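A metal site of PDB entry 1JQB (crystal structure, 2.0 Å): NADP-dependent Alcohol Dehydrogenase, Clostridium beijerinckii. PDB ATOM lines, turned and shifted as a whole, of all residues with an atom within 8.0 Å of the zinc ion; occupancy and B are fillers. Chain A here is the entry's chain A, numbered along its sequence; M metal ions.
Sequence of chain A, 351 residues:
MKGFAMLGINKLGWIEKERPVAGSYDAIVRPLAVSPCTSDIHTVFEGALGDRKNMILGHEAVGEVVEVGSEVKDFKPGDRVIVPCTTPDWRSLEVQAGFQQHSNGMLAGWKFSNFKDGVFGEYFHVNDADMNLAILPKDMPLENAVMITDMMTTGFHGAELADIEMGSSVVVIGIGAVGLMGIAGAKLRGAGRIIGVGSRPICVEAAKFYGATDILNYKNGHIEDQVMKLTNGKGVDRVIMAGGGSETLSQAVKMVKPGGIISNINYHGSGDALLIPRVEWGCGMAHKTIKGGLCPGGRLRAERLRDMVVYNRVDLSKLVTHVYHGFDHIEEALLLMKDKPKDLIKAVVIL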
ATOM      1  N   SER A  35     -19.301  27.045  16.898  1.00  0.00           N
ATOM      2  CA  SER A  35     -20.178  26.434  17.880  1.00  0.00           C
ATOM      3  C   SER A  35     -21.283  25.632  17.196  1.00  0.00           C
ATOM      4  O   SER A  35     -21.839  26.069  16.190  1.00  0.00           O
ATOM      5  CB  SER A  35     -20.807  27.509  18.772  1.00  0.00           C
ATOM      6  OG  SER A  35     -21.692  26.939  19.712  1.00  0.00           O
ATOM      7  N   PRO A  36     -21.594  24.436  17.710  1.00  0.00           N
ATOM      8  CA  PRO A  36     -22.648  23.615  17.104  1.00  0.00           C
ATOM      9  C   PRO A  36     -24.014  24.094  17.589  1.00  0.00           C
ATOM     10  O   PRO A  36     -24.135  24.593  18.706  1.00  0.00           O
ATOM     11  CB  PRO A  36     -22.316  22.212  17.599  1.00  0.00           C
ATOM     12  CG  PRO A  36     -21.750  22.471  18.963  1.00  0.00           C
ATOM     13  CD  PRO A  36     -20.855  23.677  18.730  1.00  0.00           C
ATOM     14  N   CYS A  37     -25.037  23.935  16.750  1.00  0.00           N
ATOM     15  CA  CYS A  37     -26.394  24.372  17.117  1.00  0.00           C
ATOM     16  C   CYS A  37     -27.403  23.239  17.087  1.00  0.00           C
ATOM     17  O   CYS A  37     -27.289  22.300  16.297  1.00  0.00           O
ATOM     18  CB  CYS A  37     -26.847  25.469  16.151  1.00  0.00           C
ATOM     19  SG  CYS A  37     -28.500  26.129  16.481  1.00  0.00           S
ATOM     20  N   THR A  38     -28.419  23.325  17.946  1.00  0.00           N
ATOM     21  CA  THR A  38     -29.451  22.307  17.983  1.00  0.00           C
ATOM     22  C   THR A  38     -30.111  22.208  16.603  1.00  0.00           C
ATOM     23  O   THR A  38     -30.650  21.156  16.247  1.00  0.00           O
ATOM     24  CB  THR A  38     -30.513  22.630  19.027  1.00  0.00           C
ATOM     25  OG1 THR A  38     -31.063  23.921  18.757  1.00  0.00           O
ATOM     26  CG2 THR A  38     -29.911  22.626  20.427  1.00  0.00           C
ATOM     27  N   SER A  39     -30.061  23.293  15.846  1.00  0.00           N
ATOM     28  CA  SER A  39     -30.643  23.321  14.511  1.00  0.00           C
ATOM     29  C   SER A  39     -29.946  22.320  13.598  1.00  0.00           C
ATOM     30  O   SER A  39     -30.598  21.646  12.796  1.00  0.00           O
ATOM     31  CB  SER A  39     -30.533  24.722  13.902  1.00  0.00           C
ATOM     32  OG  SER A  39     -31.263  25.668  14.670  1.00  0.00           O
ATOM     33  N   ASP A  40     -28.621  22.225  13.717  1.00  0.00           N
ATOM     34  CA  ASP A  40     -27.839  21.286  12.917  1.00  0.00           C
ATOM     35  C   ASP A  40     -28.428  19.892  13.158  1.00  0.00           C
ATOM     36  O   ASP A  40     -28.466  19.049  12.249  1.00  0.00           O
ATOM     37  CB  ASP A  40     -26.356  21.298  13.332  1.00  0.00           C
ATOM     38  CG  ASP A  40     -25.637  22.573  12.928  1.00  0.00           C
ATOM     39  OD1 ASP A  40     -25.679  22.931  11.730  1.00  0.00           O
ATOM     40  OD2 ASP A  40     -25.012  23.224  13.807  1.00  0.00           O
ATOM     41  N   GLY A  58     -22.799  23.718  10.378  1.00  0.00           N
ATOM     42  CA  GLY A  58     -22.408  24.878  11.164  1.00  0.00           C
ATOM     43  C   GLY A  58     -22.670  26.245  10.567  1.00  0.00           C
ATOM     44  O   GLY A  58     -22.506  26.468   9.371  1.00  0.00           O
ATOM     45  N   HIS A  59     -23.071  27.184  11.430  1.00  0.00           N
ATOM     46  CA  HIS A  59     -23.344  28.560  10.998  1.00  0.00           C
ATOM     47  C   HIS A  59     -23.054  29.565  12.117  1.00  0.00           C
ATOM     48  O   HIS A  59     -23.550  30.692  12.086  1.00  0.00           O
ATOM     49  CB  HIS A  59     -24.794  28.708  10.548  1.00  0.00           C
ATOM     50  CG  HIS A  59     -25.794  28.122  11.502  1.00  0.00           C
ATOM     51  ND1 HIS A  59     -26.303  26.858  11.366  1.00  0.00           N
ATOM     52  CD2 HIS A  59     -26.332  28.626  12.635  1.00  0.00           C
ATOM     53  CE1 HIS A  59     -27.117  26.600  12.374  1.00  0.00           C
ATOM     54  NE2 HIS A  59     -27.150  27.659  13.155  1.00  0.00           N
ATOM     55  N   GLU A  60     -22.276  29.156  13.107  1.00  0.00           N
ATOM     56  CA  GLU A  60     -21.912  30.049  14.205  1.00  0.00           C
ATOM     57  C   GLU A  60     -20.388  30.123  14.285  1.00  0.00           C
ATOM     58  O   GLU A  60     -19.730  29.163  14.693  1.00  0.00           O
ATOM     59  CB  GLU A  60     -22.466  29.520  15.526  1.00  0.00           C
ATOM     60  CG  GLU A  60     -23.966  29.384  15.559  1.00  0.00           C
ATOM     61  CD  GLU A  60     -24.455  28.639  16.783  1.00  0.00           C
ATOM     62  OE1 GLU A  60     -24.484  29.219  17.889  1.00  0.00           O
ATOM     63  OE2 GLU A  60     -24.798  27.458  16.650  1.00  0.00           O
ATOM     64  N   CYS A  85     -24.982  34.421  11.490  1.00  0.00           N
ATOM     65  CA  CYS A  85     -25.460  33.183  10.864  1.00  0.00           C
ATOM     66  C   CYS A  85     -26.328  33.513   9.657  1.00  0.00           C
ATOM     67  O   CYS A  85     -26.431  32.725   8.717  1.00  0.00           O
ATOM     68  CB  CYS A  85     -26.247  32.326  11.860  1.00  0.00           C
ATOM     69  SG  CYS A  85     -27.752  33.087  12.534  1.00  0.00           S
ATOM     70  N   TRP A 110     -30.715  32.899   5.584  1.00  0.00           N
ATOM     71  CA  TRP A 110     -29.864  32.020   6.373  1.00  0.00           C
ATOM     72  C   TRP A 110     -29.352  30.943   5.421  1.00  0.00           C
ATOM     73  O   TRP A 110     -30.094  30.038   5.051  1.00  0.00           O
ATOM     74  CB  TRP A 110     -30.658  31.404   7.517  1.00  0.00           C
ATOM     75  CG  TRP A 110     -30.005  30.221   8.137  1.00  0.00           C
ATOM     76  CD1 TRP A 110     -28.690  30.119   8.520  1.00  0.00           C
ATOM     77  CD2 TRP A 110     -30.605  28.957   8.427  1.00  0.00           C
ATOM     78  NE1 TRP A 110     -28.451  28.875   9.031  1.00  0.00           N
ATOM     79  CE2 TRP A 110     -29.597  28.130   8.987  1.00  0.00           C
ATOM     80  CE3 TRP A 110     -31.897  28.436   8.274  1.00  0.00           C
ATOM     81  CZ2 TRP A 110     -29.838  26.815   9.384  1.00  0.00           C
ATOM     82  CZ3 TRP A 110     -32.138  27.121   8.671  1.00  0.00           C
ATOM     83  CH2 TRP A 110     -31.112  26.331   9.220  1.00  0.00           C
ATOM     84  N   PHE A 112     -25.750  29.334   5.570  1.00  0.00           N
ATOM     85  CA  PHE A 112     -24.871  28.357   6.214  1.00  0.00           C
ATOM     86  C   PHE A 112     -25.620  27.222   6.923  1.00  0.00           C
ATOM     87  O   PHE A 112     -26.370  27.471   7.868  1.00  0.00           O
ATOM     88  CB  PHE A 112     -23.972  29.031   7.273  1.00  0.00           C
ATOM     89  CG  PHE A 112     -23.000  30.059   6.708  1.00  0.00           C
ATOM     90  CD1 PHE A 112     -22.189  29.754   5.624  1.00  0.00           C
ATOM     91  CD2 PHE A 112     -22.833  31.283   7.342  1.00  0.00           C
ATOM     92  CE1 PHE A 112     -21.211  30.651   5.185  1.00  0.00           C
ATOM     93  CE2 PHE A 112     -21.862  32.188   6.917  1.00  0.00           C
ATOM     94  CZ  PHE A 112     -21.045  31.863   5.831  1.00  0.00           C
ATOM     95  N   SER A 113     -25.402  25.994   6.468  1.00  0.00           N
ATOM     96  CA  SER A 113     -26.051  24.843   7.105  1.00  0.00           C
ATOM     97  C   SER A 113     -27.528  24.704   6.740  1.00  0.00           C
ATOM     98  O   SER A 113     -28.206  23.785   7.199  1.00  0.00           O
ATOM     99  CB  SER A 113     -25.899  24.943   8.626  1.00  0.00           C
ATOM    100  OG  SER A 113     -26.646  23.948   9.291  1.00  0.00           O
ATOM    101  N   THR A 149     -23.365  35.638  16.879  1.00  0.00           N
ATOM    102  CA  THR A 149     -23.788  35.179  15.559  1.00  0.00           C
ATOM    103  C   THR A 149     -25.133  34.493  15.417  1.00  0.00           C
ATOM    104  O   THR A 149     -25.731  34.523  14.338  1.00  0.00           O
ATOM    105  CB  THR A 149     -22.729  34.233  14.949  1.00  0.00           C
ATOM    106  OG1 THR A 149     -22.713  33.001  15.691  1.00  0.00           O
ATOM    107  CG2 THR A 149     -21.356  34.879  15.018  1.00  0.00           C
ATOM    108  N   ASP A 150     -25.611  33.875  16.498  1.00  0.00           N
ATOM    109  CA  ASP A 150     -26.880  33.166  16.435  1.00  0.00           C
ATOM    110  C   ASP A 150     -27.718  33.263  17.719  1.00  0.00           C
ATOM    111  O   ASP A 150     -28.879  33.688  17.683  1.00  0.00           O
ATOM    112  CB  ASP A 150     -26.606  31.706  16.115  1.00  0.00           C
ATOM    113  CG  ASP A 150     -27.871  30.914  15.862  1.00  0.00           C
ATOM    114  OD1 ASP A 150     -28.973  31.481  15.889  1.00  0.00           O
ATOM    115  OD2 ASP A 150     -27.735  29.700  15.624  1.00  0.00           O
ATOM    116  N   MET A 151     -27.125  32.872  18.848  1.00  0.00           N
ATOM    117  CA  MET A 151     -27.849  32.880  20.113  1.00  0.00           C
ATOM    118  C   MET A 151     -28.384  34.265  20.512  1.00  0.00           C
ATOM    119  O   MET A 151     -29.576  34.399  20.812  1.00  0.00           O
ATOM    120  CB  MET A 151     -26.959  32.321  21.220  1.00  0.00           C
ATOM    121  CG  MET A 151     -26.466  30.894  20.982  1.00  0.00           C
ATOM    122  SD  MET A 151     -27.768  29.671  20.731  1.00  0.00           S
ATOM    123  CE  MET A 151     -27.836  29.642  18.956  1.00  0.00           C
ATOM    124  N   THR A 154     -30.857  35.768  17.837  1.00  0.00           N
ATOM    125  CA  THR A 154     -32.113  35.018  17.826  1.00  0.00           C
ATOM    126  C   THR A 154     -32.942  35.309  19.070  1.00  0.00           C
ATOM    127  O   THR A 154     -34.111  35.673  18.966  1.00  0.00           O
ATOM    128  CB  THR A 154     -31.848  33.501  17.730  1.00  0.00           C
ATOM    129  OG1 THR A 154     -31.155  33.220  16.497  1.00  0.00           O
ATOM    130  CG2 THR A 154     -33.149  32.727  17.728  1.00  0.00           C
ATOM    131  N   VAL A 178     -30.861  29.907  23.426  1.00  0.00           N
ATOM    132  CA  VAL A 178     -31.788  30.818  22.774  1.00  0.00           C
ATOM    133  C   VAL A 178     -32.810  31.409  23.751  1.00  0.00           C
ATOM    134  O   VAL A 178     -33.095  32.603  23.705  1.00  0.00           O
ATOM    135  CB  VAL A 178     -32.558  30.126  21.632  1.00  0.00           C
ATOM    136  CG1 VAL A 178     -33.623  31.061  21.077  1.00  0.00           C
ATOM    137  CG2 VAL A 178     -31.569  29.719  20.537  1.00  0.00           C
ATOM    138  N   TYR A 267     -37.084  26.769  16.277  1.00  0.00           N
ATOM    139  CA  TYR A 267     -37.046  26.108  14.968  1.00  0.00           C
ATOM    140  C   TYR A 267     -37.765  24.771  15.138  1.00  0.00           C
ATOM    141  O   TYR A 267     -37.227  23.838  15.712  1.00  0.00           O
ATOM    142  CB  TYR A 267     -35.578  25.929  14.560  1.00  0.00           C
ATOM    143  CG  TYR A 267     -35.273  25.019  13.388  1.00  0.00           C
ATOM    144  CD1 TYR A 267     -36.264  24.600  12.500  1.00  0.00           C
ATOM    145  CD2 TYR A 267     -33.969  24.579  13.162  1.00  0.00           C
ATOM    146  CE1 TYR A 267     -35.961  23.747  11.422  1.00  0.00           C
ATOM    147  CE2 TYR A 267     -33.652  23.740  12.099  1.00  0.00           C
ATOM    148  CZ  TYR A 267     -34.648  23.329  11.234  1.00  0.00           C
ATOM    149  OH  TYR A 267     -34.326  22.479  10.202  1.00  0.00           O
ATOM    150  N   LEU A 294     -37.090  34.184  11.726  1.00  0.00           N
ATOM    151  CA  LEU A 294     -35.670  33.847  11.641  1.00  0.00           C
ATOM    152  C   LEU A 294     -34.881  35.053  12.143  1.00  0.00           C
ATOM    153  O   LEU A 294     -35.255  36.199  11.877  1.00  0.00           O
ATOM    154  CB  LEU A 294     -35.301  33.581  10.192  1.00  0.00           C
ATOM    155  CG  LEU A 294     -33.822  33.467   9.806  1.00  0.00           C
ATOM    156  CD1 LEU A 294     -33.187  32.255  10.469  1.00  0.00           C
ATOM    157  CD2 LEU A 294     -33.719  33.362   8.291  1.00  0.00           C
ATOM    158  N   CYS A 295     -33.794  34.798  12.857  1.00  0.00           N
ATOM    159  CA  CYS A 295     -32.975  35.885  13.388  1.00  0.00           C
ATOM    160  C   CYS A 295     -32.401  36.776  12.292  1.00  0.00           C
ATOM    161  O   CYS A 295     -32.015  36.305  11.229  1.00  0.00           O
ATOM    162  CB  CYS A 295     -31.816  35.321  14.214  1.00  0.00           C
ATOM    163  SG  CYS A 295     -30.592  34.426  13.231  1.00  0.00           S
ATOM    164  N   LYS A 346     -23.874  25.897  25.837  1.00  0.00           N
ATOM    165  CA  LYS A 346     -23.257  26.037  24.518  1.00  0.00           C
ATOM    166  C   LYS A 346     -21.778  25.627  24.565  1.00  0.00           C
ATOM    167  O   LYS A 346     -21.086  25.830  25.567  1.00  0.00           O
ATOM    168  CB  LYS A 346     -23.366  27.479  24.015  1.00  0.00           C
ATOM    169  CG  LYS A 346     -24.756  27.887  23.565  1.00  0.00           C
ATOM    170  CD  LYS A 346     -25.171  27.199  22.269  1.00  0.00           C
ATOM    171  CE  LYS A 346     -24.468  27.780  21.045  1.00  0.00           C
ATOM    172  NZ  LYS A 346     -25.040  27.208  19.793  1.00  0.00           N
HETATM  173 ZN    ZN M   1     -28.398  28.031  14.920  1.00  0.00          ZN
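The side-chain hydroxyl (OG1) of Thr 154 lies within hydrogen-bond range of the backbone carbonyl oxygen (O) of Asp 150 (2.6 Å). The side-chain sulfur of Cys 37 sits close to the backbone NH of Ser 39 (3.3 Å). The side-chain carboxylate (OD2) of Asp 40 lies within hydrogen-bond range of the backbone NH (N) of Cys 37 (3.0 Å).
Residues that only touch the zinc ion: Ser 39 (3.7 Å). Four residues have an atom within 4 Å of the zinc ion: Cys 37, Ser 39, His 59 and Asp 150.
The zinc ion is bound by the side-chain carboxylate of Asp 150 (1.9 Å), a ring nitrogen (NE2) of His 59 (2.2 Å) and the side-chain sulfur of Cys 37 (2.5 Å).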
